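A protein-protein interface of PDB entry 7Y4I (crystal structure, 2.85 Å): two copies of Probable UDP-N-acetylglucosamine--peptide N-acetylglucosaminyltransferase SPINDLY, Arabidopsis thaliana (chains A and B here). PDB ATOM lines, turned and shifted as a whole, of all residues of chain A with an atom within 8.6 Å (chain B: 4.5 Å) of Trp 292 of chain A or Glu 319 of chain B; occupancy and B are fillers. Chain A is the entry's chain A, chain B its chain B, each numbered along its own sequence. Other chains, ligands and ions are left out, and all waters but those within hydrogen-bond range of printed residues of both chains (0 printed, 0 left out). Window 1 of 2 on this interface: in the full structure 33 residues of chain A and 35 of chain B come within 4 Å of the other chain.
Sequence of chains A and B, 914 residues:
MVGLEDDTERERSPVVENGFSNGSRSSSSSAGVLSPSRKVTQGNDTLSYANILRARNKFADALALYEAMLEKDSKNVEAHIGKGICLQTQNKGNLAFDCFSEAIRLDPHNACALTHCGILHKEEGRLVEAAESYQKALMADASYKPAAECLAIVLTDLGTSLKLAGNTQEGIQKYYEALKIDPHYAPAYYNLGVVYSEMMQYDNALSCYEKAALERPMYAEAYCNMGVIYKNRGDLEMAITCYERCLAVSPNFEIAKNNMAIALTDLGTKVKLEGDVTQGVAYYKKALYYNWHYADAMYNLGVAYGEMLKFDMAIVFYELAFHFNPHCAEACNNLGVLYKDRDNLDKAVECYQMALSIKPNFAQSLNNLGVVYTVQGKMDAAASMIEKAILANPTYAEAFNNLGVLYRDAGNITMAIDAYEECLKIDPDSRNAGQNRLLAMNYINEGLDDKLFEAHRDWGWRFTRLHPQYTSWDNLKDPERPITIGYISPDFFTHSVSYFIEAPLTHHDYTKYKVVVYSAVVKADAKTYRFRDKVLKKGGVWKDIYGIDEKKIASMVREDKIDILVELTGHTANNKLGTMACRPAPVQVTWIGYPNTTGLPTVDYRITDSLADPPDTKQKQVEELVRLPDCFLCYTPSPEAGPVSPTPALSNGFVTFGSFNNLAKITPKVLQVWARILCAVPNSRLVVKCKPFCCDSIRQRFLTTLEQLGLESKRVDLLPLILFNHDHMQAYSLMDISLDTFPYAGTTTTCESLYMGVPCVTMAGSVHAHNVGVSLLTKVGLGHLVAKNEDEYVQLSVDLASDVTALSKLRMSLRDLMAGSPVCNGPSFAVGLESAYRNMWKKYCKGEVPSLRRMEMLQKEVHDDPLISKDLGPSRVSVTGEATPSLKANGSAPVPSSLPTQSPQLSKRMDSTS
OE2 of Glu 319 of chain B is in salt-bridge range of NZ of Lys 347 of chain B, 3.9 Å away.
Among the printed residues, pairs that only touch across the chains: Lys 257 of chain A with Lys 347 of chain B (3.6 Å), Leu 288 of chain A with Val 316 of chain B (3.4 Å), Tyr 289 of chain A with Ile 315 of chain B (3.8 Å), Tyr 289 of chain A with Val 316 of chain B (3.8 Å), Trp 292 of chain A with Glu 319 of chain B (3.6 Å), Trp 292 of chain A with Leu 320 of chain B (3.98 Å), Trp 292 of chain A with His 323 of chain B (3.6 Å), His 323 of chain A with His 323 of chain B (2.9 Å), Phe 324 of chain A with Leu 320 of chain B (3.8 Å) and Phe 324 of chain A with His 323 of chain B (3.3 Å).
Of the printed residues of chain B, Lys 257 of chain A touches Lys 347. Lys 285 of chain A touches none of the printed residues of chain B. Of the printed residues of chain B, Trp 292 of chain A touches Glu 319 (3.6 Å), Leu 320 (3.98 Å) and His 323 (3.6 Å). Of the printed residues of chain B, His 323 of chain A touches His 323 (2.9 Å). Of the printed residues of chain A, Ile 315 of chain B touches Tyr 289 (3.8 Å). Glu 319 of chain B touches just one residue of chain A: Trp 292. Of the printed residues of chain A, Lys 347 of chain B touches Lys 257. The nearest printed residue of chain A that does not touch Ile 315 of chain B is Trp 292 of chain A (5.7 Å).
Hydrophobic or aromatic side chains of chain A that line the printed part of chain B: Leu 288, Tyr 289, Trp 292, His 323 and Phe 324. Among the printed residues, 10 pairs touch across the chains. Among the printed residues, no Asp or Glu carboxylate lies within 4 Å of a Lys or Arg side-chain nitrogen of the other chain.
His 323 of chain A touches its own counterpart, His 323 of chain B. Positions printed for both chains: 320, 321 and 323. Of the 10 pairs that touch across the chains among the printed residues, 1 has its exchanged pair printed and touching as well.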
ATOM      1  N   GLU A 254     -15.354  23.081 -21.728  1.00  0.00           N
ATOM      2  CA  GLU A 254     -16.647  22.903 -21.073  1.00  0.00           C
ATOM      3  C   GLU A 254     -16.612  23.339 -19.615  1.00  0.00           C
ATOM      4  O   GLU A 254     -17.511  24.048 -19.153  1.00  0.00           O
ATOM      5  CB  GLU A 254     -17.107  21.450 -21.194  1.00  0.00           C
ATOM      6  CG  GLU A 254     -18.274  21.265 -22.157  1.00  0.00           C
ATOM      7  CD  GLU A 254     -19.547  21.928 -21.664  1.00  0.00           C
ATOM      8  OE1 GLU A 254     -20.372  22.336 -22.510  1.00  0.00           O
ATOM      9  OE2 GLU A 254     -19.726  22.040 -20.432  1.00  0.00           O
ATOM     10  N   LYS A 257     -16.648  26.853 -19.382  1.00  0.00           N
ATOM     11  CA  LYS A 257     -17.977  27.381 -19.674  1.00  0.00           C
ATOM     12  C   LYS A 257     -18.881  27.295 -18.450  1.00  0.00           C
ATOM     13  O   LYS A 257     -19.569  28.263 -18.108  1.00  0.00           O
ATOM     14  CB  LYS A 257     -18.593  26.628 -20.853  1.00  0.00           C
ATOM     15  CG  LYS A 257     -18.101  27.093 -22.208  1.00  0.00           C
ATOM     16  CD  LYS A 257     -18.599  26.179 -23.303  1.00  0.00           C
ATOM     17  CE  LYS A 257     -20.117  26.120 -23.302  1.00  0.00           C
ATOM     18  NZ  LYS A 257     -20.646  25.748 -24.642  1.00  0.00           N
ATOM     19  N   ASN A 258     -18.896  26.136 -17.781  1.00  0.00           N
ATOM     20  CA  ASN A 258     -19.701  25.979 -16.573  1.00  0.00           C
ATOM     21  C   ASN A 258     -19.261  26.952 -15.491  1.00  0.00           C
ATOM     22  O   ASN A 258     -20.098  27.556 -14.807  1.00  0.00           O
ATOM     23  CB  ASN A 258     -19.603  24.543 -16.059  1.00  0.00           C
ATOM     24  CG  ASN A 258     -20.096  23.527 -17.066  1.00  0.00           C
ATOM     25  OD1 ASN A 258     -20.590  23.883 -18.136  1.00  0.00           O
ATOM     26  ND2 ASN A 258     -19.957  22.250 -16.729  1.00  0.00           N
ATOM     27  N   ALA A 261     -20.659  30.363 -16.181  1.00  0.00           N
ATOM     28  CA  ALA A 261     -22.059  30.527 -15.809  1.00  0.00           C
ATOM     29  C   ALA A 261     -22.212  30.696 -14.304  1.00  0.00           C
ATOM     30  O   ALA A 261     -23.030  31.501 -13.842  1.00  0.00           O
ATOM     31  CB  ALA A 261     -22.881  29.339 -16.310  1.00  0.00           C
ATOM     32  N   TYR A 284     -27.752  36.778 -15.556  1.00  0.00           N
ATOM     33  CA  TYR A 284     -28.396  35.469 -15.517  1.00  0.00           C
ATOM     34  C   TYR A 284     -28.602  34.919 -16.921  1.00  0.00           C
ATOM     35  O   TYR A 284     -28.376  33.729 -17.172  1.00  0.00           O
ATOM     36  CB  TYR A 284     -29.736  35.557 -14.790  1.00  0.00           C
ATOM     37  CG  TYR A 284     -29.657  35.890 -13.316  1.00  0.00           C
ATOM     38  CD1 TYR A 284     -28.629  35.399 -12.519  1.00  0.00           C
ATOM     39  CD2 TYR A 284     -30.628  36.686 -12.719  1.00  0.00           C
ATOM     40  CE1 TYR A 284     -28.568  35.701 -11.169  1.00  0.00           C
ATOM     41  CE2 TYR A 284     -30.574  36.995 -11.377  1.00  0.00           C
ATOM     42  CZ  TYR A 284     -29.544  36.503 -10.606  1.00  0.00           C
ATOM     43  OH  TYR A 284     -29.502  36.813  -9.266  1.00  0.00           O
ATOM     44  N   LYS A 285     -29.018  35.777 -17.855  1.00  0.00           N
ATOM     45  CA  LYS A 285     -29.260  35.322 -19.219  1.00  0.00           C
ATOM     46  C   LYS A 285     -27.960  34.952 -19.918  1.00  0.00           C
ATOM     47  O   LYS A 285     -27.907  33.951 -20.642  1.00  0.00           O
ATOM     48  CB  LYS A 285     -30.010  36.396 -20.006  1.00  0.00           C
ATOM     49  CG  LYS A 285     -31.472  36.542 -19.613  1.00  0.00           C
ATOM     50  CD  LYS A 285     -32.167  37.569 -20.486  1.00  0.00           C
ATOM     51  CE  LYS A 285     -33.536  37.936 -19.934  1.00  0.00           C
ATOM     52  NZ  LYS A 285     -34.263  38.862 -20.853  1.00  0.00           N
ATOM     53  N   LYS A 286     -26.903  35.745 -19.725  1.00  0.00           N
ATOM     54  CA  LYS A 286     -25.623  35.399 -20.334  1.00  0.00           C
ATOM     55  C   LYS A 286     -25.071  34.104 -19.754  1.00  0.00           C
ATOM     56  O   LYS A 286     -24.445  33.315 -20.471  1.00  0.00           O
ATOM     57  CB  LYS A 286     -24.623  36.542 -20.168  1.00  0.00           C
ATOM     58  CG  LYS A 286     -23.527  36.533 -21.227  1.00  0.00           C
ATOM     59  CD  LYS A 286     -23.049  37.935 -21.572  1.00  0.00           C
ATOM     60  CE  LYS A 286     -23.382  38.296 -23.014  1.00  0.00           C
ATOM     61  NZ  LYS A 286     -23.104  39.731 -23.304  1.00  0.00           N
ATOM     62  N   ALA A 287     -25.297  33.866 -18.459  1.00  0.00           N
ATOM     63  CA  ALA A 287     -24.962  32.571 -17.873  1.00  0.00           C
ATOM     64  C   ALA A 287     -25.638  31.440 -18.635  1.00  0.00           C
ATOM     65  O   ALA A 287     -25.016  30.407 -18.918  1.00  0.00           O
ATOM     66  CB  ALA A 287     -25.359  32.541 -16.397  1.00  0.00           C
ATOM     67  N   LEU A 288     -26.908  31.624 -18.995  1.00  0.00           N
ATOM     68  CA  LEU A 288     -27.630  30.600 -19.735  1.00  0.00           C
ATOM     69  C   LEU A 288     -27.064  30.395 -21.133  1.00  0.00           C
ATOM     70  O   LEU A 288     -27.266  29.327 -21.718  1.00  0.00           O
ATOM     71  CB  LEU A 288     -29.117  30.958 -19.814  1.00  0.00           C
ATOM     72  CG  LEU A 288     -29.892  31.003 -18.496  1.00  0.00           C
ATOM     73  CD1 LEU A 288     -31.315  31.452 -18.744  1.00  0.00           C
ATOM     74  CD2 LEU A 288     -29.869  29.650 -17.802  1.00  0.00           C
ATOM     75  N   TYR A 289     -26.366  31.387 -21.689  1.00  0.00           N
ATOM     76  CA  TYR A 289     -25.693  31.166 -22.963  1.00  0.00           C
ATOM     77  C   TYR A 289     -24.500  30.232 -22.794  1.00  0.00           C
ATOM     78  O   TYR A 289     -24.236  29.392 -23.661  1.00  0.00           O
ATOM     79  CB  TYR A 289     -25.255  32.500 -23.564  1.00  0.00           C
ATOM     80  CG  TYR A 289     -24.118  32.397 -24.552  1.00  0.00           C
ATOM     81  CD1 TYR A 289     -24.278  31.735 -25.760  1.00  0.00           C
ATOM     82  CD2 TYR A 289     -22.884  32.967 -24.279  1.00  0.00           C
ATOM     83  CE1 TYR A 289     -23.238  31.639 -26.667  1.00  0.00           C
ATOM     84  CE2 TYR A 289     -21.841  32.880 -25.179  1.00  0.00           C
ATOM     85  CZ  TYR A 289     -22.023  32.215 -26.372  1.00  0.00           C
ATOM     86  OH  TYR A 289     -20.986  32.124 -27.268  1.00  0.00           O
ATOM     87  N   TYR A 290     -23.779  30.353 -21.674  1.00  0.00           N
ATOM     88  CA  TYR A 290     -22.653  29.461 -21.407  1.00  0.00           C
ATOM     89  C   TYR A 290     -23.118  28.103 -20.892  1.00  0.00           C
ATOM     90  O   TYR A 290     -22.505  27.074 -21.204  1.00  0.00           O
ATOM     91  CB  TYR A 290     -21.690  30.113 -20.414  1.00  0.00           C
ATOM     92  CG  TYR A 290     -20.932  31.273 -21.011  1.00  0.00           C
ATOM     93  CD1 TYR A 290     -19.813  31.062 -21.803  1.00  0.00           C
ATOM     94  CD2 TYR A 290     -21.351  32.582 -20.802  1.00  0.00           C
ATOM     95  CE1 TYR A 290     -19.123  32.122 -22.359  1.00  0.00           C
ATOM     96  CE2 TYR A 290     -20.670  33.648 -21.355  1.00  0.00           C
ATOM     97  CZ  TYR A 290     -19.556  33.414 -22.132  1.00  0.00           C
ATOM     98  OH  TYR A 290     -18.872  34.474 -22.683  1.00  0.00           O
ATOM     99  N   ASN A 291     -24.194  28.077 -20.110  1.00  0.00           N
ATOM    100  CA  ASN A 291     -24.772  26.827 -19.615  1.00  0.00           C
ATOM    101  C   ASN A 291     -26.288  26.973 -19.715  1.00  0.00           C
ATOM    102  O   ASN A 291     -26.912  27.608 -18.860  1.00  0.00           O
ATOM    103  CB  ASN A 291     -24.323  26.535 -18.189  1.00  0.00           C
ATOM    104  CG  ASN A 291     -24.796  25.180 -17.690  1.00  0.00           C
ATOM    105  OD1 ASN A 291     -25.548  24.478 -18.370  1.00  0.00           O
ATOM    106  ND2 ASN A 291     -24.359  24.807 -16.491  1.00  0.00           N
ATOM    107  N   TRP A 292     -26.877  26.376 -20.757  1.00  0.00           N
ATOM    108  CA  TRP A 292     -28.304  26.548 -20.993  1.00  0.00           C
ATOM    109  C   TRP A 292     -29.164  25.789 -19.998  1.00  0.00           C
ATOM    110  O   TRP A 292     -30.370  26.047 -19.930  1.00  0.00           O
ATOM    111  CB  TRP A 292     -28.671  26.138 -22.423  1.00  0.00           C
ATOM    112  CG  TRP A 292     -28.341  24.716 -22.801  1.00  0.00           C
ATOM    113  CD1 TRP A 292     -27.223  24.281 -23.449  1.00  0.00           C
ATOM    114  CD2 TRP A 292     -29.155  23.552 -22.588  1.00  0.00           C
ATOM    115  NE1 TRP A 292     -27.282  22.922 -23.642  1.00  0.00           N
ATOM    116  CE2 TRP A 292     -28.456  22.450 -23.119  1.00  0.00           C
ATOM    117  CE3 TRP A 292     -30.399  23.336 -21.992  1.00  0.00           C
ATOM    118  CZ2 TRP A 292     -28.959  21.155 -23.073  1.00  0.00           C
ATOM    119  CZ3 TRP A 292     -30.898  22.047 -21.947  1.00  0.00           C
ATOM    120  CH2 TRP A 292     -30.180  20.973 -22.485  1.00  0.00           C
ATOM    121  N   HIS A 293     -28.588  24.873 -19.223  1.00  0.00           N
ATOM    122  CA  HIS A 293     -29.341  24.148 -18.210  1.00  0.00           C
ATOM    123  C   HIS A 293     -28.819  24.439 -16.809  1.00  0.00           C
ATOM    124  O   HIS A 293     -28.906  23.589 -15.920  1.00  0.00           O
ATOM    125  CB  HIS A 293     -29.320  22.645 -18.490  1.00  0.00           C
ATOM    126  CG  HIS A 293     -27.951  22.040 -18.451  1.00  0.00           C
ATOM    127  ND1 HIS A 293     -27.058  22.154 -19.493  1.00  0.00           N
ATOM    128  CD2 HIS A 293     -27.328  21.307 -17.499  1.00  0.00           C
ATOM    129  CE1 HIS A 293     -25.940  21.521 -19.183  1.00  0.00           C
ATOM    130  NE2 HIS A 293     -26.079  20.998 -17.978  1.00  0.00           N
ATOM    131  N   TYR A 294     -28.288  25.640 -16.587  1.00  0.00           N
ATOM    132  CA  TYR A 294     -27.847  26.021 -15.248  1.00  0.00           C
ATOM    133  C   TYR A 294     -29.076  26.424 -14.446  1.00  0.00           C
ATOM    134  O   TYR A 294     -29.575  27.545 -14.569  1.00  0.00           O
ATOM    135  CB  TYR A 294     -26.822  27.148 -15.299  1.00  0.00           C
ATOM    136  CG  TYR A 294     -26.160  27.383 -13.959  1.00  0.00           C
ATOM    137  CD1 TYR A 294     -25.958  26.332 -13.075  1.00  0.00           C
ATOM    138  CD2 TYR A 294     -25.752  28.652 -13.572  1.00  0.00           C
ATOM    139  CE1 TYR A 294     -25.362  26.535 -11.849  1.00  0.00           C
ATOM    140  CE2 TYR A 294     -25.149  28.864 -12.345  1.00  0.00           C
ATOM    141  CZ  TYR A 294     -24.958  27.801 -11.486  1.00  0.00           C
ATOM    142  OH  TYR A 294     -24.359  28.002 -10.261  1.00  0.00           O
ATOM    143  N   ALA A 295     -29.553  25.503 -13.603  1.00  0.00           N
ATOM    144  CA  ALA A 295     -30.811  25.717 -12.894  1.00  0.00           C
ATOM    145  C   ALA A 295     -30.764  26.961 -12.016  1.00  0.00           C
ATOM    146  O   ALA A 295     -31.763  27.678 -11.896  1.00  0.00           O
ATOM    147  CB  ALA A 295     -31.156  24.485 -12.061  1.00  0.00           C
ATOM    148  N   ALA A 297     -29.391  29.875 -12.400  1.00  0.00           N
ATOM    149  CA  ALA A 297     -29.738  31.090 -13.129  1.00  0.00           C
ATOM    150  C   ALA A 297     -31.212  31.115 -13.500  1.00  0.00           C
ATOM    151  O   ALA A 297     -31.824  32.186 -13.537  1.00  0.00           O
ATOM    152  CB  ALA A 297     -28.871  31.226 -14.380  1.00  0.00           C
ATOM    153  N   MET A 298     -31.795  29.949 -13.777  1.00  0.00           N
ATOM    154  CA  MET A 298     -33.211  29.889 -14.114  1.00  0.00           C
ATOM    155  C   MET A 298     -34.080  30.262 -12.917  1.00  0.00           C
ATOM    156  O   MET A 298     -35.039  31.033 -13.049  1.00  0.00           O
ATOM    157  CB  MET A 298     -33.557  28.493 -14.623  1.00  0.00           C
ATOM    158  CG  MET A 298     -34.371  28.494 -15.890  1.00  0.00           C
ATOM    159  SD  MET A 298     -33.293  28.398 -17.314  1.00  0.00           S
ATOM    160  CE  MET A 298     -32.777  26.691 -17.180  1.00  0.00           C
ATOM    161  N   LEU A 320     -38.637  25.545 -15.348  1.00  0.00           N
ATOM    162  CA  LEU A 320     -37.382  25.092 -15.939  1.00  0.00           C
ATOM    163  C   LEU A 320     -36.334  24.820 -14.868  1.00  0.00           C
ATOM    164  O   LEU A 320     -35.575  23.849 -14.964  1.00  0.00           O
ATOM    165  CB  LEU A 320     -36.869  26.129 -16.941  1.00  0.00           C
ATOM    166  CG  LEU A 320     -37.650  26.296 -18.247  1.00  0.00           C
ATOM    167  CD1 LEU A 320     -37.037  27.401 -19.094  1.00  0.00           C
ATOM    168  CD2 LEU A 320     -37.705  24.982 -19.022  1.00  0.00           C
ATOM    169  N   ALA A 321     -36.280  25.663 -13.835  1.00  0.00           N
ATOM    170  CA  ALA A 321     -35.310  25.456 -12.765  1.00  0.00           C
ATOM    171  C   ALA A 321     -35.571  24.141 -12.043  1.00  0.00           C
ATOM    172  O   ALA A 321     -34.648  23.352 -11.811  1.00  0.00           O
ATOM    173  CB  ALA A 321     -35.347  26.630 -11.789  1.00  0.00           C
ATOM    174  N   HIS A 323     -37.165  21.641 -13.233  1.00  0.00           N
ATOM    175  CA  HIS A 323     -36.968  20.549 -14.182  1.00  0.00           C
ATOM    176  C   HIS A 323     -35.503  20.128 -14.244  1.00  0.00           C
ATOM    177  O   HIS A 323     -35.191  18.932 -14.222  1.00  0.00           O
ATOM    178  CB  HIS A 323     -37.477  20.966 -15.560  1.00  0.00           C
ATOM    179  CG  HIS A 323     -37.127  20.005 -16.648  1.00  0.00           C
ATOM    180  ND1 HIS A 323     -36.157  20.271 -17.590  1.00  0.00           N
ATOM    181  CD2 HIS A 323     -37.611  18.776 -16.942  1.00  0.00           C
ATOM    182  CE1 HIS A 323     -36.061  19.248 -18.419  1.00  0.00           C
ATOM    183  NE2 HIS A 323     -36.933  18.328 -18.050  1.00  0.00           N
ATOM    184  N   PHE A 324     -34.588  21.097 -14.310  1.00  0.00           N
ATOM    185  CA  PHE A 324     -33.161  20.800 -14.370  1.00  0.00           C
ATOM    186  C   PHE A 324     -32.548  20.541 -13.000  1.00  0.00           C
ATOM    187  O   PHE A 324     -31.409  20.069 -12.929  1.00  0.00           O
ATOM    188  CB  PHE A 324     -32.411  21.941 -15.065  1.00  0.00           C
ATOM    189  CG  PHE A 324     -32.762  22.096 -16.513  1.00  0.00           C
ATOM    190  CD1 PHE A 324     -32.622  21.033 -17.390  1.00  0.00           C
ATOM    191  CD2 PHE A 324     -33.251  23.293 -16.994  1.00  0.00           C
ATOM    192  CE1 PHE A 324     -32.955  21.168 -18.724  1.00  0.00           C
ATOM    193  CE2 PHE A 324     -33.586  23.436 -18.327  1.00  0.00           C
ATOM    194  CZ  PHE A 324     -33.437  22.371 -19.194  1.00  0.00           C
ATOM    195  N   ILE B 315     -29.758  31.291 -28.947  1.00  0.00           N
ATOM    196  CA  ILE B 315     -29.045  30.034 -28.731  1.00  0.00           C
ATOM    197  C   ILE B 315     -29.675  29.261 -27.578  1.00  0.00           C
ATOM    198  O   ILE B 315     -29.824  28.033 -27.641  1.00  0.00           O
ATOM    199  CB  ILE B 315     -27.549  30.308 -28.489  1.00  0.00           C
ATOM    200  CG1 ILE B 315     -26.858  30.671 -29.804  1.00  0.00           C
ATOM    201  CG2 ILE B 315     -26.861  29.110 -27.835  1.00  0.00           C
ATOM    202  CD1 ILE B 315     -25.357  30.851 -29.670  1.00  0.00           C
ATOM    203  N   VAL B 316     -30.059  29.964 -26.509  1.00  0.00           N
ATOM    204  CA  VAL B 316     -30.662  29.295 -25.359  1.00  0.00           C
ATOM    205  C   VAL B 316     -31.994  28.668 -25.746  1.00  0.00           C
ATOM    206  O   VAL B 316     -32.263  27.499 -25.440  1.00  0.00           O
ATOM    207  CB  VAL B 316     -30.825  30.277 -24.184  1.00  0.00           C
ATOM    208  CG1 VAL B 316     -31.468  29.573 -23.002  1.00  0.00           C
ATOM    209  CG2 VAL B 316     -29.479  30.859 -23.783  1.00  0.00           C
ATOM    210  N   PHE B 317     -32.854  29.439 -26.416  1.00  0.00           N
ATOM    211  CA  PHE B 317     -34.154  28.912 -26.822  1.00  0.00           C
ATOM    212  C   PHE B 317     -34.001  27.669 -27.689  1.00  0.00           C
ATOM    213  O   PHE B 317     -34.767  26.708 -27.549  1.00  0.00           O
ATOM    214  CB  PHE B 317     -34.951  29.987 -27.559  1.00  0.00           C
ATOM    215  CG  PHE B 317     -35.588  31.004 -26.651  1.00  0.00           C
ATOM    216  CD1 PHE B 317     -36.395  30.607 -25.597  1.00  0.00           C
ATOM    217  CD2 PHE B 317     -35.376  32.360 -26.852  1.00  0.00           C
ATOM    218  CE1 PHE B 317     -36.984  31.546 -24.761  1.00  0.00           C
ATOM    219  CE2 PHE B 317     -35.958  33.303 -26.021  1.00  0.00           C
ATOM    220  CZ  PHE B 317     -36.765  32.895 -24.975  1.00  0.00           C
ATOM    221  N   TYR B 318     -33.010  27.664 -28.584  1.00  0.00           N
ATOM    222  CA  TYR B 318     -32.813  26.520 -29.470  1.00  0.00           C
ATOM    223  C   TYR B 318     -32.377  25.285 -28.691  1.00  0.00           C
ATOM    224  O   TYR B 318     -32.887  24.183 -28.923  1.00  0.00           O
ATOM    225  CB  TYR B 318     -31.778  26.861 -30.538  1.00  0.00           C
ATOM    226  CG  TYR B 318     -32.278  27.747 -31.653  1.00  0.00           C
ATOM    227  CD1 TYR B 318     -33.494  27.508 -32.273  1.00  0.00           C
ATOM    228  CD2 TYR B 318     -31.519  28.819 -32.093  1.00  0.00           C
ATOM    229  CE1 TYR B 318     -33.940  28.320 -33.300  1.00  0.00           C
ATOM    230  CE2 TYR B 318     -31.954  29.634 -33.109  1.00  0.00           C
ATOM    231  CZ  TYR B 318     -33.161  29.382 -33.712  1.00  0.00           C
ATOM    232  OH  TYR B 318     -33.578  30.201 -34.731  1.00  0.00           O
ATOM    233  N   GLU B 319     -31.420  25.448 -27.772  1.00  0.00           N
ATOM    234  CA  GLU B 319     -30.983  24.312 -26.966  1.00  0.00           C
ATOM    235  C   GLU B 319     -32.134  23.764 -26.136  1.00  0.00           C
ATOM    236  O   GLU B 319     -32.264  22.546 -25.966  1.00  0.00           O
ATOM    237  CB  GLU B 319     -29.810  24.713 -26.067  1.00  0.00           C
ATOM    238  CG  GLU B 319     -28.575  25.187 -26.820  1.00  0.00           C
ATOM    239  CD  GLU B 319     -27.595  24.063 -27.119  1.00  0.00           C
ATOM    240  OE1 GLU B 319     -28.042  22.978 -27.551  1.00  0.00           O
ATOM    241  OE2 GLU B 319     -26.376  24.270 -26.931  1.00  0.00           O
ATOM    242  N   LEU B 320     -32.994  24.652 -25.631  1.00  0.00           N
ATOM    243  CA  LEU B 320     -34.168  24.212 -24.885  1.00  0.00           C
ATOM    244  C   LEU B 320     -35.149  23.472 -25.788  1.00  0.00           C
ATOM    245  O   LEU B 320     -35.736  22.465 -25.376  1.00  0.00           O
ATOM    246  CB  LEU B 320     -34.846  25.407 -24.215  1.00  0.00           C
ATOM    247  CG  LEU B 320     -34.148  25.989 -22.985  1.00  0.00           C
ATOM    248  CD1 LEU B 320     -34.878  27.221 -22.480  1.00  0.00           C
ATOM    249  CD2 LEU B 320     -34.035  24.940 -21.895  1.00  0.00           C
ATOM    250  N   ALA B 321     -35.349  23.960 -27.015  1.00  0.00           N
ATOM    251  CA  ALA B 321     -36.214  23.256 -27.959  1.00  0.00           C
ATOM    252  C   ALA B 321     -35.678  21.861 -28.248  1.00  0.00           C
ATOM    253  O   ALA B 321     -36.417  20.872 -28.182  1.00  0.00           O
ATOM    254  CB  ALA B 321     -36.349  24.053 -29.257  1.00  0.00           C
ATOM    255  N   PHE B 322     -34.383  21.764 -28.561  1.00  0.00           N
ATOM    256  CA  PHE B 322     -33.793  20.468 -28.869  1.00  0.00           C
ATOM    257  C   PHE B 322     -33.723  19.576 -27.638  1.00  0.00           C
ATOM    258  O   PHE B 322     -33.730  18.346 -27.766  1.00  0.00           O
ATOM    259  CB  PHE B 322     -32.401  20.655 -29.474  1.00  0.00           C
ATOM    260  CG  PHE B 322     -31.699  19.365 -29.774  1.00  0.00           C
ATOM    261  CD1 PHE B 322     -32.262  18.442 -30.634  1.00  0.00           C
ATOM    262  CD2 PHE B 322     -30.482  19.073 -29.196  1.00  0.00           C
ATOM    263  CE1 PHE B 322     -31.620  17.253 -30.912  1.00  0.00           C
ATOM    264  CE2 PHE B 322     -29.834  17.885 -29.473  1.00  0.00           C
ATOM    265  CZ  PHE B 322     -30.405  16.976 -30.331  1.00  0.00           C
ATOM    266  N   HIS B 323     -33.646  20.171 -26.444  1.00  0.00           N
ATOM    267  CA  HIS B 323     -33.657  19.372 -25.222  1.00  0.00           C
ATOM    268  C   HIS B 323     -34.989  18.658 -25.048  1.00  0.00           C
ATOM    269  O   HIS B 323     -35.029  17.453 -24.771  1.00  0.00           O
ATOM    270  CB  HIS B 323     -33.363  20.252 -24.011  1.00  0.00           C
ATOM    271  CG  HIS B 323     -33.599  19.569 -22.703  1.00  0.00           C
ATOM    272  ND1 HIS B 323     -32.819  18.523 -22.260  1.00  0.00           N
ATOM    273  CD2 HIS B 323     -34.530  19.777 -21.743  1.00  0.00           C
ATOM    274  CE1 HIS B 323     -33.257  18.118 -21.080  1.00  0.00           C
ATOM    275  NE2 HIS B 323     -34.294  18.862 -20.745  1.00  0.00           N
ATOM    276  N   LEU B 335     -28.723  26.491 -34.593  1.00  0.00           N
ATOM    277  CA  LEU B 335     -27.605  26.618 -33.666  1.00  0.00           C
ATOM    278  C   LEU B 335     -26.274  26.582 -34.410  1.00  0.00           C
ATOM    279  O   LEU B 335     -25.363  27.366 -34.112  1.00  0.00           O
ATOM    280  CB  LEU B 335     -27.664  25.505 -32.618  1.00  0.00           C
ATOM    281  CG  LEU B 335     -28.480  25.771 -31.355  1.00  0.00           C
ATOM    282  CD1 LEU B 335     -28.832  24.464 -30.672  1.00  0.00           C
ATOM    283  CD2 LEU B 335     -27.717  26.680 -30.412  1.00  0.00           C
ATOM    284  N   LYS B 347     -18.026  23.673 -32.939  1.00  0.00           N
ATOM    285  CA  LYS B 347     -19.385  23.465 -32.447  1.00  0.00           C
ATOM    286  C   LYS B 347     -20.407  23.556 -33.573  1.00  0.00           C
ATOM    287  O   LYS B 347     -21.423  22.850 -33.545  1.00  0.00           O
ATOM    288  CB  LYS B 347     -19.709  24.469 -31.338  1.00  0.00           C
ATOM    289  CG  LYS B 347     -21.125  24.357 -30.792  1.00  0.00           C
ATOM    290  CD  LYS B 347     -21.174  24.567 -29.282  1.00  0.00           C
ATOM    291  CE  LYS B 347     -22.249  23.702 -28.636  1.00  0.00           C
ATOM    292  NZ  LYS B 347     -22.507  24.082 -27.220  1.00  0.00           N
